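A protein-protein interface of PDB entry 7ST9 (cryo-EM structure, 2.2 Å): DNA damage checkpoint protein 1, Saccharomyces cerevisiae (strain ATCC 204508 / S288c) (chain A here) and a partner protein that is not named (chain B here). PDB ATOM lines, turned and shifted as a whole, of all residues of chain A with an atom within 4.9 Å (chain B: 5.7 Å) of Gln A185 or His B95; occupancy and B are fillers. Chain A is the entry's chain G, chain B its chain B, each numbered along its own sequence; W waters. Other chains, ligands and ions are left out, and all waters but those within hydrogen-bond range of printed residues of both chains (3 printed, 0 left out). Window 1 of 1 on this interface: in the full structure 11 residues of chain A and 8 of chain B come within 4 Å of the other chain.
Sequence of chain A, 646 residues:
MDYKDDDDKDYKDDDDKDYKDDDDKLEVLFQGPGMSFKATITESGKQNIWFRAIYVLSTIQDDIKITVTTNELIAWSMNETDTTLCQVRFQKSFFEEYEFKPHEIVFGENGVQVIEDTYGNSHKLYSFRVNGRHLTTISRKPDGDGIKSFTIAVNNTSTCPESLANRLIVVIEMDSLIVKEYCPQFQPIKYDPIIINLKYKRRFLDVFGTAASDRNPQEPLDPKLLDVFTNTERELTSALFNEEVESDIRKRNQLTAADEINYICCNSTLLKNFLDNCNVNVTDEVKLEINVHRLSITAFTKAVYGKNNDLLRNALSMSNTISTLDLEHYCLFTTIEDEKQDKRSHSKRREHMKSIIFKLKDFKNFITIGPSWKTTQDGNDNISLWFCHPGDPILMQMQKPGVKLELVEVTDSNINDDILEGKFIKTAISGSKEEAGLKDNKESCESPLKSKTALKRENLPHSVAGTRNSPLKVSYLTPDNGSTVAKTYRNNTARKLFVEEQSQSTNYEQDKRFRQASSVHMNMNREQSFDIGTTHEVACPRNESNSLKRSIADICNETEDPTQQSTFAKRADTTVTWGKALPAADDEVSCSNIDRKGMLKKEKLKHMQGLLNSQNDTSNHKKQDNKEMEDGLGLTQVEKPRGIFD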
ATOM      1  N   ARG A 129      32.863   9.035 -23.639  1.00  0.00           N
ATOM      2  CA  ARG A 129      31.606   8.441 -23.209  1.00  0.00           C
ATOM      3  C   ARG A 129      30.506   8.845 -24.180  1.00  0.00           C
ATOM      4  O   ARG A 129      30.455   9.997 -24.621  1.00  0.00           O
ATOM      5  CB  ARG A 129      31.257   8.891 -21.786  1.00  0.00           C
ATOM      6  CG  ARG A 129      29.896   8.445 -21.302  1.00  0.00           C
ATOM      7  CD  ARG A 129      29.725   8.704 -19.811  1.00  0.00           C
ATOM      8  NE  ARG A 129      29.935  10.105 -19.464  1.00  0.00           N
ATOM      9  CZ  ARG A 129      28.997  11.043 -19.512  1.00  0.00           C
ATOM     10  NH1 ARG A 129      27.762  10.770 -19.900  1.00  0.00           N
ATOM     11  NH2 ARG A 129      29.307  12.288 -19.159  1.00  0.00           N
ATOM     12  N   VAL A 130      29.632   7.900 -24.518  1.00  0.00           N
ATOM     13  CA  VAL A 130      28.566   8.144 -25.483  1.00  0.00           C
ATOM     14  C   VAL A 130      27.297   7.441 -25.019  1.00  0.00           C
ATOM     15  O   VAL A 130      27.350   6.340 -24.463  1.00  0.00           O
ATOM     16  CB  VAL A 130      28.967   7.676 -26.899  1.00  0.00           C
ATOM     17  CG1 VAL A 130      29.124   6.161 -26.942  1.00  0.00           C
ATOM     18  CG2 VAL A 130      27.944   8.145 -27.925  1.00  0.00           C
ATOM     19  N   ASN A 131      26.154   8.080 -25.255  1.00  0.00           N
ATOM     20  CA  ASN A 131      24.870   7.486 -24.907  1.00  0.00           C
ATOM     21  C   ASN A 131      24.711   6.131 -25.590  1.00  0.00           C
ATOM     22  O   ASN A 131      24.755   6.035 -26.820  1.00  0.00           O
ATOM     23  CB  ASN A 131      23.737   8.428 -25.309  1.00  0.00           C
ATOM     24  CG  ASN A 131      22.373   7.909 -24.901  1.00  0.00           C
ATOM     25  OD1 ASN A 131      21.876   6.930 -25.459  1.00  0.00           O
ATOM     26  ND2 ASN A 131      21.759   8.566 -23.926  1.00  0.00           N
ATOM     27  N   ARG A 133      22.063   4.011 -25.756  1.00  0.00           N
ATOM     28  CA  ARG A 133      20.836   3.800 -26.516  1.00  0.00           C
ATOM     29  C   ARG A 133      20.922   4.452 -27.891  1.00  0.00           C
ATOM     30  O   ARG A 133      20.489   3.867 -28.892  1.00  0.00           O
ATOM     31  CB  ARG A 133      19.637   4.344 -25.740  1.00  0.00           C
ATOM     32  CG  ARG A 133      19.334   3.577 -24.465  1.00  0.00           C
ATOM     33  CD  ARG A 133      17.932   3.862 -23.950  1.00  0.00           C
ATOM     34  NE  ARG A 133      17.605   5.283 -23.974  1.00  0.00           N
ATOM     35  CZ  ARG A 133      18.142   6.193 -23.172  1.00  0.00           C
ATOM     36  NH1 ARG A 133      19.054   5.869 -22.271  1.00  0.00           N
ATOM     37  NH2 ARG A 133      17.757   7.462 -23.282  1.00  0.00           N
ATOM     38  N   HIS A 134      21.476   5.663 -27.959  1.00  0.00           N
ATOM     39  CA  HIS A 134      21.602   6.351 -29.239  1.00  0.00           C
ATOM     40  C   HIS A 134      22.504   5.573 -30.189  1.00  0.00           C
ATOM     41  O   HIS A 134      22.179   5.393 -31.369  1.00  0.00           O
ATOM     42  CB  HIS A 134      22.139   7.764 -29.013  1.00  0.00           C
ATOM     43  CG  HIS A 134      21.190   8.660 -28.281  1.00  0.00           C
ATOM     44  ND1 HIS A 134      21.539   9.920 -27.847  1.00  0.00           N
ATOM     45  CD2 HIS A 134      19.903   8.475 -27.902  1.00  0.00           C
ATOM     46  CE1 HIS A 134      20.509  10.474 -27.233  1.00  0.00           C
ATOM     47  NE2 HIS A 134      19.504   9.619 -27.254  1.00  0.00           N
ATOM     48  N   ASN A 166      33.632  17.473 -30.363  1.00  0.00           N
ATOM     49  CA  ASN A 166      33.117  16.508 -29.391  1.00  0.00           C
ATOM     50  C   ASN A 166      31.860  15.813 -29.913  1.00  0.00           C
ATOM     51  O   ASN A 166      30.863  15.664 -29.206  1.00  0.00           O
ATOM     52  CB  ASN A 166      32.848  17.184 -28.043  1.00  0.00           C
ATOM     53  CG  ASN A 166      34.122  17.602 -27.338  1.00  0.00           C
ATOM     54  OD1 ASN A 166      35.161  16.956 -27.475  1.00  0.00           O
ATOM     55  ND2 ASN A 166      34.050  18.688 -26.580  1.00  0.00           N
ATOM     56  N   ARG A 167      31.917  15.387 -31.174  1.00  0.00           N
ATOM     57  CA  ARG A 167      30.838  14.621 -31.781  1.00  0.00           C
ATOM     58  C   ARG A 167      31.424  13.455 -32.562  1.00  0.00           C
ATOM     59  O   ARG A 167      32.441  13.602 -33.245  1.00  0.00           O
ATOM     60  CB  ARG A 167      29.977  15.492 -32.703  1.00  0.00           C
ATOM     61  CG  ARG A 167      29.046  16.434 -31.960  1.00  0.00           C
ATOM     62  CD  ARG A 167      28.466  17.489 -32.884  1.00  0.00           C
ATOM     63  NE  ARG A 167      27.193  18.000 -32.390  1.00  0.00           N
ATOM     64  CZ  ARG A 167      26.681  19.181 -32.711  1.00  0.00           C
ATOM     65  NH1 ARG A 167      27.300  20.001 -33.546  1.00  0.00           N
ATOM     66  NH2 ARG A 167      25.517  19.548 -32.183  1.00  0.00           N
ATOM     67  N   CYS A 183      25.729  12.534 -35.876  1.00  0.00           N
ATOM     68  CA  CYS A 183      26.805  13.138 -35.085  1.00  0.00           C
ATOM     69  C   CYS A 183      26.384  13.215 -33.623  1.00  0.00           C
ATOM     70  O   CYS A 183      26.182  14.303 -33.072  1.00  0.00           O
ATOM     71  CB  CYS A 183      27.168  14.521 -35.628  1.00  0.00           C
ATOM     72  SG  CYS A 183      25.756  15.514 -36.154  1.00  0.00           S
ATOM     73  N   PRO A 184      26.237  12.069 -32.960  1.00  0.00           N
ATOM     74  CA  PRO A 184      25.948  12.090 -31.520  1.00  0.00           C
ATOM     75  C   PRO A 184      27.099  12.694 -30.727  1.00  0.00           C
ATOM     76  O   PRO A 184      28.272  12.476 -31.030  1.00  0.00           O
ATOM     77  CB  PRO A 184      25.739  10.610 -31.176  1.00  0.00           C
ATOM     78  CG  PRO A 184      26.404   9.857 -32.278  1.00  0.00           C
ATOM     79  CD  PRO A 184      26.237  10.700 -33.500  1.00  0.00           C
ATOM     80  N   GLN A 185      26.750  13.440 -29.683  1.00  0.00           N
ATOM     81  CA  GLN A 185      27.755  14.071 -28.838  1.00  0.00           C
ATOM     82  C   GLN A 185      28.452  13.038 -27.958  1.00  0.00           C
ATOM     83  O   GLN A 185      27.869  12.022 -27.568  1.00  0.00           O
ATOM     84  CB  GLN A 185      27.112  15.147 -27.964  1.00  0.00           C
ATOM     85  CG  GLN A 185      26.176  14.602 -26.895  1.00  0.00           C
ATOM     86  CD  GLN A 185      25.411  15.695 -26.175  1.00  0.00           C
ATOM     87  OE1 GLN A 185      25.174  16.769 -26.728  1.00  0.00           O
ATOM     88  NE2 GLN A 185      25.026  15.430 -24.933  1.00  0.00           N
ATOM     89  N   PHE A 186      29.719  13.306 -27.643  1.00  0.00           N
ATOM     90  CA  PHE A 186      30.476  12.482 -26.712  1.00  0.00           C
ATOM     91  C   PHE A 186      31.273  13.376 -25.773  1.00  0.00           C
ATOM     92  O   PHE A 186      31.604  14.517 -26.107  1.00  0.00           O
ATOM     93  CB  PHE A 186      31.412  11.499 -27.438  1.00  0.00           C
ATOM     94  CG  PHE A 186      32.575  12.152 -28.142  1.00  0.00           C
ATOM     95  CD1 PHE A 186      33.711  12.529 -27.442  1.00  0.00           C
ATOM     96  CD2 PHE A 186      32.541  12.361 -29.510  1.00  0.00           C
ATOM     97  CE1 PHE A 186      34.779  13.118 -28.089  1.00  0.00           C
ATOM     98  CE2 PHE A 186      33.609  12.948 -30.162  1.00  0.00           C
ATOM     99  CZ  PHE A 186      34.729  13.324 -29.451  1.00  0.00           C
ATOM    100  N   GLN A 187      31.580  12.841 -24.590  1.00  0.00           N
ATOM    101  CA  GLN A 187      32.329  13.560 -23.570  1.00  0.00           C
ATOM    102  C   GLN A 187      33.672  12.880 -23.346  1.00  0.00           C
ATOM    103  O   GLN A 187      33.696  11.694 -22.986  1.00  0.00           O
ATOM    104  CB  GLN A 187      31.540  13.617 -22.263  1.00  0.00           C
ATOM    105  CG  GLN A 187      30.265  14.437 -22.349  1.00  0.00           C
ATOM    106  CD  GLN A 187      29.062  13.608 -22.751  1.00  0.00           C
ATOM    107  OE1 GLN A 187      28.869  12.497 -22.260  1.00  0.00           O
ATOM    108  NE2 GLN A 187      28.247  14.145 -23.654  1.00  0.00           N
ATOM    109  N   ARG B  90      14.817  13.627 -17.600  1.00  0.00           N
ATOM    110  CA  ARG B  90      15.671  12.450 -17.686  1.00  0.00           C
ATOM    111  C   ARG B  90      16.519  12.447 -18.952  1.00  0.00           C
ATOM    112  O   ARG B  90      17.657  11.967 -18.924  1.00  0.00           O
ATOM    113  CB  ARG B  90      14.820  11.180 -17.628  1.00  0.00           C
ATOM    114  CG  ARG B  90      14.360  10.791 -16.231  1.00  0.00           C
ATOM    115  CD  ARG B  90      14.078   9.299 -16.140  1.00  0.00           C
ATOM    116  NE  ARG B  90      13.096   8.980 -15.110  1.00  0.00           N
ATOM    117  CZ  ARG B  90      11.799   8.805 -15.327  1.00  0.00           C
ATOM    118  NH1 ARG B  90      11.274   8.913 -16.537  1.00  0.00           N
ATOM    119  NH2 ARG B  90      11.004   8.515 -14.300  1.00  0.00           N
ATOM    120  N   ASN B  91      15.994  12.962 -20.065  1.00  0.00           N
ATOM    121  CA  ASN B  91      16.684  12.847 -21.345  1.00  0.00           C
ATOM    122  C   ASN B  91      17.232  14.173 -21.858  1.00  0.00           C
ATOM    123  O   ASN B  91      18.450  14.326 -21.973  1.00  0.00           O
ATOM    124  CB  ASN B  91      15.732  12.234 -22.383  1.00  0.00           C
ATOM    125  CG  ASN B  91      15.424  10.775 -22.100  1.00  0.00           C
ATOM    126  OD1 ASN B  91      16.202   9.887 -22.446  1.00  0.00           O
ATOM    127  ND2 ASN B  91      14.286  10.524 -21.465  1.00  0.00           N
ATOM    128  N   GLN B  92      16.379  15.167 -22.107  1.00  0.00           N
ATOM    129  CA  GLN B  92      16.830  16.354 -22.830  1.00  0.00           C
ATOM    130  C   GLN B  92      17.716  17.232 -21.953  1.00  0.00           C
ATOM    131  O   GLN B  92      18.830  17.600 -22.348  1.00  0.00           O
ATOM    132  CB  GLN B  92      15.624  17.147 -23.335  1.00  0.00           C
ATOM    133  CG  GLN B  92      15.972  18.229 -24.344  1.00  0.00           C
ATOM    134  CD  GLN B  92      14.780  19.093 -24.711  1.00  0.00           C
ATOM    135  OE1 GLN B  92      13.648  18.799 -24.333  1.00  0.00           O
ATOM    136  NE2 GLN B  92      15.032  20.165 -25.451  1.00  0.00           N
ATOM    137  N   ILE B  93      17.232  17.584 -20.761  1.00  0.00           N
ATOM    138  CA  ILE B  93      18.018  18.416 -19.857  1.00  0.00           C
ATOM    139  C   ILE B  93      19.294  17.693 -19.451  1.00  0.00           C
ATOM    140  O   ILE B  93      20.366  18.301 -19.358  1.00  0.00           O
ATOM    141  CB  ILE B  93      17.176  18.817 -18.632  1.00  0.00           C
ATOM    142  CG1 ILE B  93      16.066  19.784 -19.052  1.00  0.00           C
ATOM    143  CG2 ILE B  93      18.057  19.444 -17.559  1.00  0.00           C
ATOM    144  CD1 ILE B  93      14.951  19.918 -18.042  1.00  0.00           C
ATOM    145  N   LYS B  94      19.197  16.386 -19.195  1.00  0.00           N
ATOM    146  CA  LYS B  94      20.375  15.618 -18.809  1.00  0.00           C
ATOM    147  C   LYS B  94      21.427  15.633 -19.913  1.00  0.00           C
ATOM    148  O   LYS B  94      22.617  15.839 -19.648  1.00  0.00           O
ATOM    149  CB  LYS B  94      19.970  14.182 -18.467  1.00  0.00           C
ATOM    150  CG  LYS B  94      21.124  13.292 -18.028  1.00  0.00           C
ATOM    151  CD  LYS B  94      20.660  11.864 -17.784  1.00  0.00           C
ATOM    152  CE  LYS B  94      21.835  10.911 -17.657  1.00  0.00           C
ATOM    153  NZ  LYS B  94      22.656  11.194 -16.448  1.00  0.00           N
ATOM    154  N   HIS B  95      21.007  15.421 -21.162  1.00  0.00           N
ATOM    155  CA  HIS B  95      21.963  15.418 -22.265  1.00  0.00           C
ATOM    156  C   HIS B  95      22.562  16.802 -22.477  1.00  0.00           C
ATOM    157  O   HIS B  95      23.758  16.927 -22.764  1.00  0.00           O
ATOM    158  CB  HIS B  95      21.288  14.916 -23.540  1.00  0.00           C
ATOM    159  CG  HIS B  95      20.790  13.507 -23.441  1.00  0.00           C
ATOM    160  ND1 HIS B  95      19.660  13.069 -24.098  1.00  0.00           N
ATOM    161  CD2 HIS B  95      21.264  12.440 -22.754  1.00  0.00           C
ATOM    162  CE1 HIS B  95      19.462  11.792 -23.823  1.00  0.00           C
ATOM    163  NE2 HIS B  95      20.420  11.387 -23.009  1.00  0.00           N
ATOM    164  N   PHE B  96      21.752  17.854 -22.338  1.00  0.00           N
ATOM    165  CA  PHE B  96      22.289  19.205 -22.462  1.00  0.00           C
ATOM    166  C   PHE B  96      23.321  19.487 -21.377  1.00  0.00           C
ATOM    167  O   PHE B  96      24.378  20.068 -21.649  1.00  0.00           O
ATOM    168  CB  PHE B  96      21.157  20.230 -22.404  1.00  0.00           C
ATOM    169  CG  PHE B  96      21.627  21.655 -22.495  1.00  0.00           C
ATOM    170  CD1 PHE B  96      22.057  22.180 -23.703  1.00  0.00           C
ATOM    171  CD2 PHE B  96      21.643  22.468 -21.374  1.00  0.00           C
ATOM    172  CE1 PHE B  96      22.491  23.490 -23.790  1.00  0.00           C
ATOM    173  CE2 PHE B  96      22.076  23.777 -21.455  1.00  0.00           C
ATOM    174  CZ  PHE B  96      22.500  24.289 -22.666  1.00  0.00           C
ATOM    175  N   ALA B  97      23.037  19.076 -20.138  1.00  0.00           N
ATOM    176  CA  ALA B  97      23.973  19.309 -19.044  1.00  0.00           C
ATOM    177  C   ALA B  97      25.233  18.467 -19.193  1.00  0.00           C
ATOM    178  O   ALA B  97      26.308  18.879 -18.741  1.00  0.00           O
ATOM    179  CB  ALA B  97      23.297  19.017 -17.704  1.00  0.00           C
ATOM    180  N   GLN B  98      25.125  17.292 -19.815  1.00  0.00           N
ATOM    181  CA  GLN B  98      26.293  16.454 -20.051  1.00  0.00           C
ATOM    182  C   GLN B  98      27.160  16.963 -21.195  1.00  0.00           C
ATOM    183  O   GLN B  98      28.330  16.581 -21.284  1.00  0.00           O
ATOM    184  CB  GLN B  98      25.859  15.018 -20.354  1.00  0.00           C
ATOM    185  CG  GLN B  98      25.451  14.216 -19.132  1.00  0.00           C
ATOM    186  CD  GLN B  98      24.860  12.866 -19.493  1.00  0.00           C
ATOM    187  OE1 GLN B  98      24.197  12.721 -20.520  1.00  0.00           O
ATOM    188  NE2 GLN B  98      25.099  11.870 -18.650  1.00  0.00           N
ATOM    189  N   LYS B  99      26.615  17.811 -22.065  1.00  0.00           N
ATOM    190  CA  LYS B  99      27.353  18.258 -23.238  1.00  0.00           C
ATOM    191  C   LYS B  99      28.627  18.989 -22.830  1.00  0.00           C
ATOM    192  O   LYS B  99      28.625  19.818 -21.918  1.00  0.00           O
ATOM    193  CB  LYS B  99      26.475  19.172 -24.092  1.00  0.00           C
ATOM    194  CG  LYS B  99      26.992  19.388 -25.502  1.00  0.00           C
ATOM    195  CD  LYS B  99      26.633  20.769 -26.025  1.00  0.00           C
ATOM    196  CE  LYS B  99      25.129  20.977 -26.080  1.00  0.00           C
ATOM    197  NZ  LYS B  99      24.772  22.275 -26.713  1.00  0.00           N
HETATM  198  O   HOH W   1      22.461  17.886 -25.821  1.00  0.00           O
HETATM  199  O   HOH W   2      14.927   7.152 -23.065  1.00  0.00           O
HETATM  200  O   HOH W   3      24.312  10.019 -22.108  1.00  0.00           O
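A ring nitrogen (ND1) of His B95 sits at hydrogen-bond distance from the backbone carbonyl oxygen (O) of Asn B91 (2.7 Å). NE2 of Gln B98 lies close to NZ of Lys B94 (3.4 Å). The backbone carbonyl oxygen (O) of Gln A187 is in hydrogen-bond range of the backbone NH (N) of Arg A129. The side-chain amide oxygen (OD1) of Asn A131 is in hydrogen-bond range of the backbone NH (N) of Arg A133 (2.9 Å). The side-chain amide oxygen of Asn A131 is in hydrogen-bond range of the backbone NH of His A134 (2.8 Å).
The guanidinium group (NH2) of Arg A133 sits at hydrogen-bond distance from the side-chain amide oxygen (OD1) of Asn B91 (3.0 Å). The side-chain amide nitrogen (ND2) of Asn A131 is in hydrogen-bond range of a ring nitrogen (NE2) of His B95, at 3.3 Å. The side-chain amide nitrogen (NE2) of Gln A185 is in hydrogen-bond range of the backbone carbonyl oxygen (O) of His B95 (2.9 Å). NE2 of Gln B98 lies close to NH1 of Arg A129, 3.1 Å away. The backbone carbonyl oxygen (O) of Gln B98 sits close to the side-chain amide nitrogen (NE2) of Gln A187 (3.4 Å).
Of the 12 printed residues of chain A, 6 touch a printed residue of chain B. Hydrophobic or aromatic side chains of chain A within 4 Å of the printed part of chain B: His A134. Of the 10 printed residues of chain B, 4 touch a printed residue of chain A. Among the printed residues, no Asp or Glu carboxylate lies within 4 Å of a Lys or Arg side-chain nitrogen of the other chain.
Gln A185 touches just these residues of chain B: His B95 and Lys B99. Of chain A, only Asn A131 (3.3 Å), His A134 (3.8 Å) and Gln A185 (2.9 Å) come within 4 Å of His B95. Of the printed residues of chain B, Asn A131 touches His B95. Printed residues of chain B within 4 Å of Arg A133: Asn B91 (3.0 Å). Of the printed residues of chain A, Lys B99 touches Gln A185. Ala B97 touches none of the printed residues of chain A. The nearest printed residue of chain A that does not touch Gln B98 is Gln A185 (4.6 Å).
Water W2 lies within hydrogen-bond range of NH2 of Arg A133 (2.9 Å) and OD1 of Asn B91 (3.1 Å). Water W1 bridges the side-chain amide oxygen of Gln A185 and the backbone carbonyl oxygen of His B95. Water W3 lies within hydrogen-bond range of OE1 of Gln B98 (3.1 Å) and ND2 of Asn A131 (3.5 Å).
His A134 touches His B95. Lys B99 touches Gln A185 (CG to OE1, 3.4 Å).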
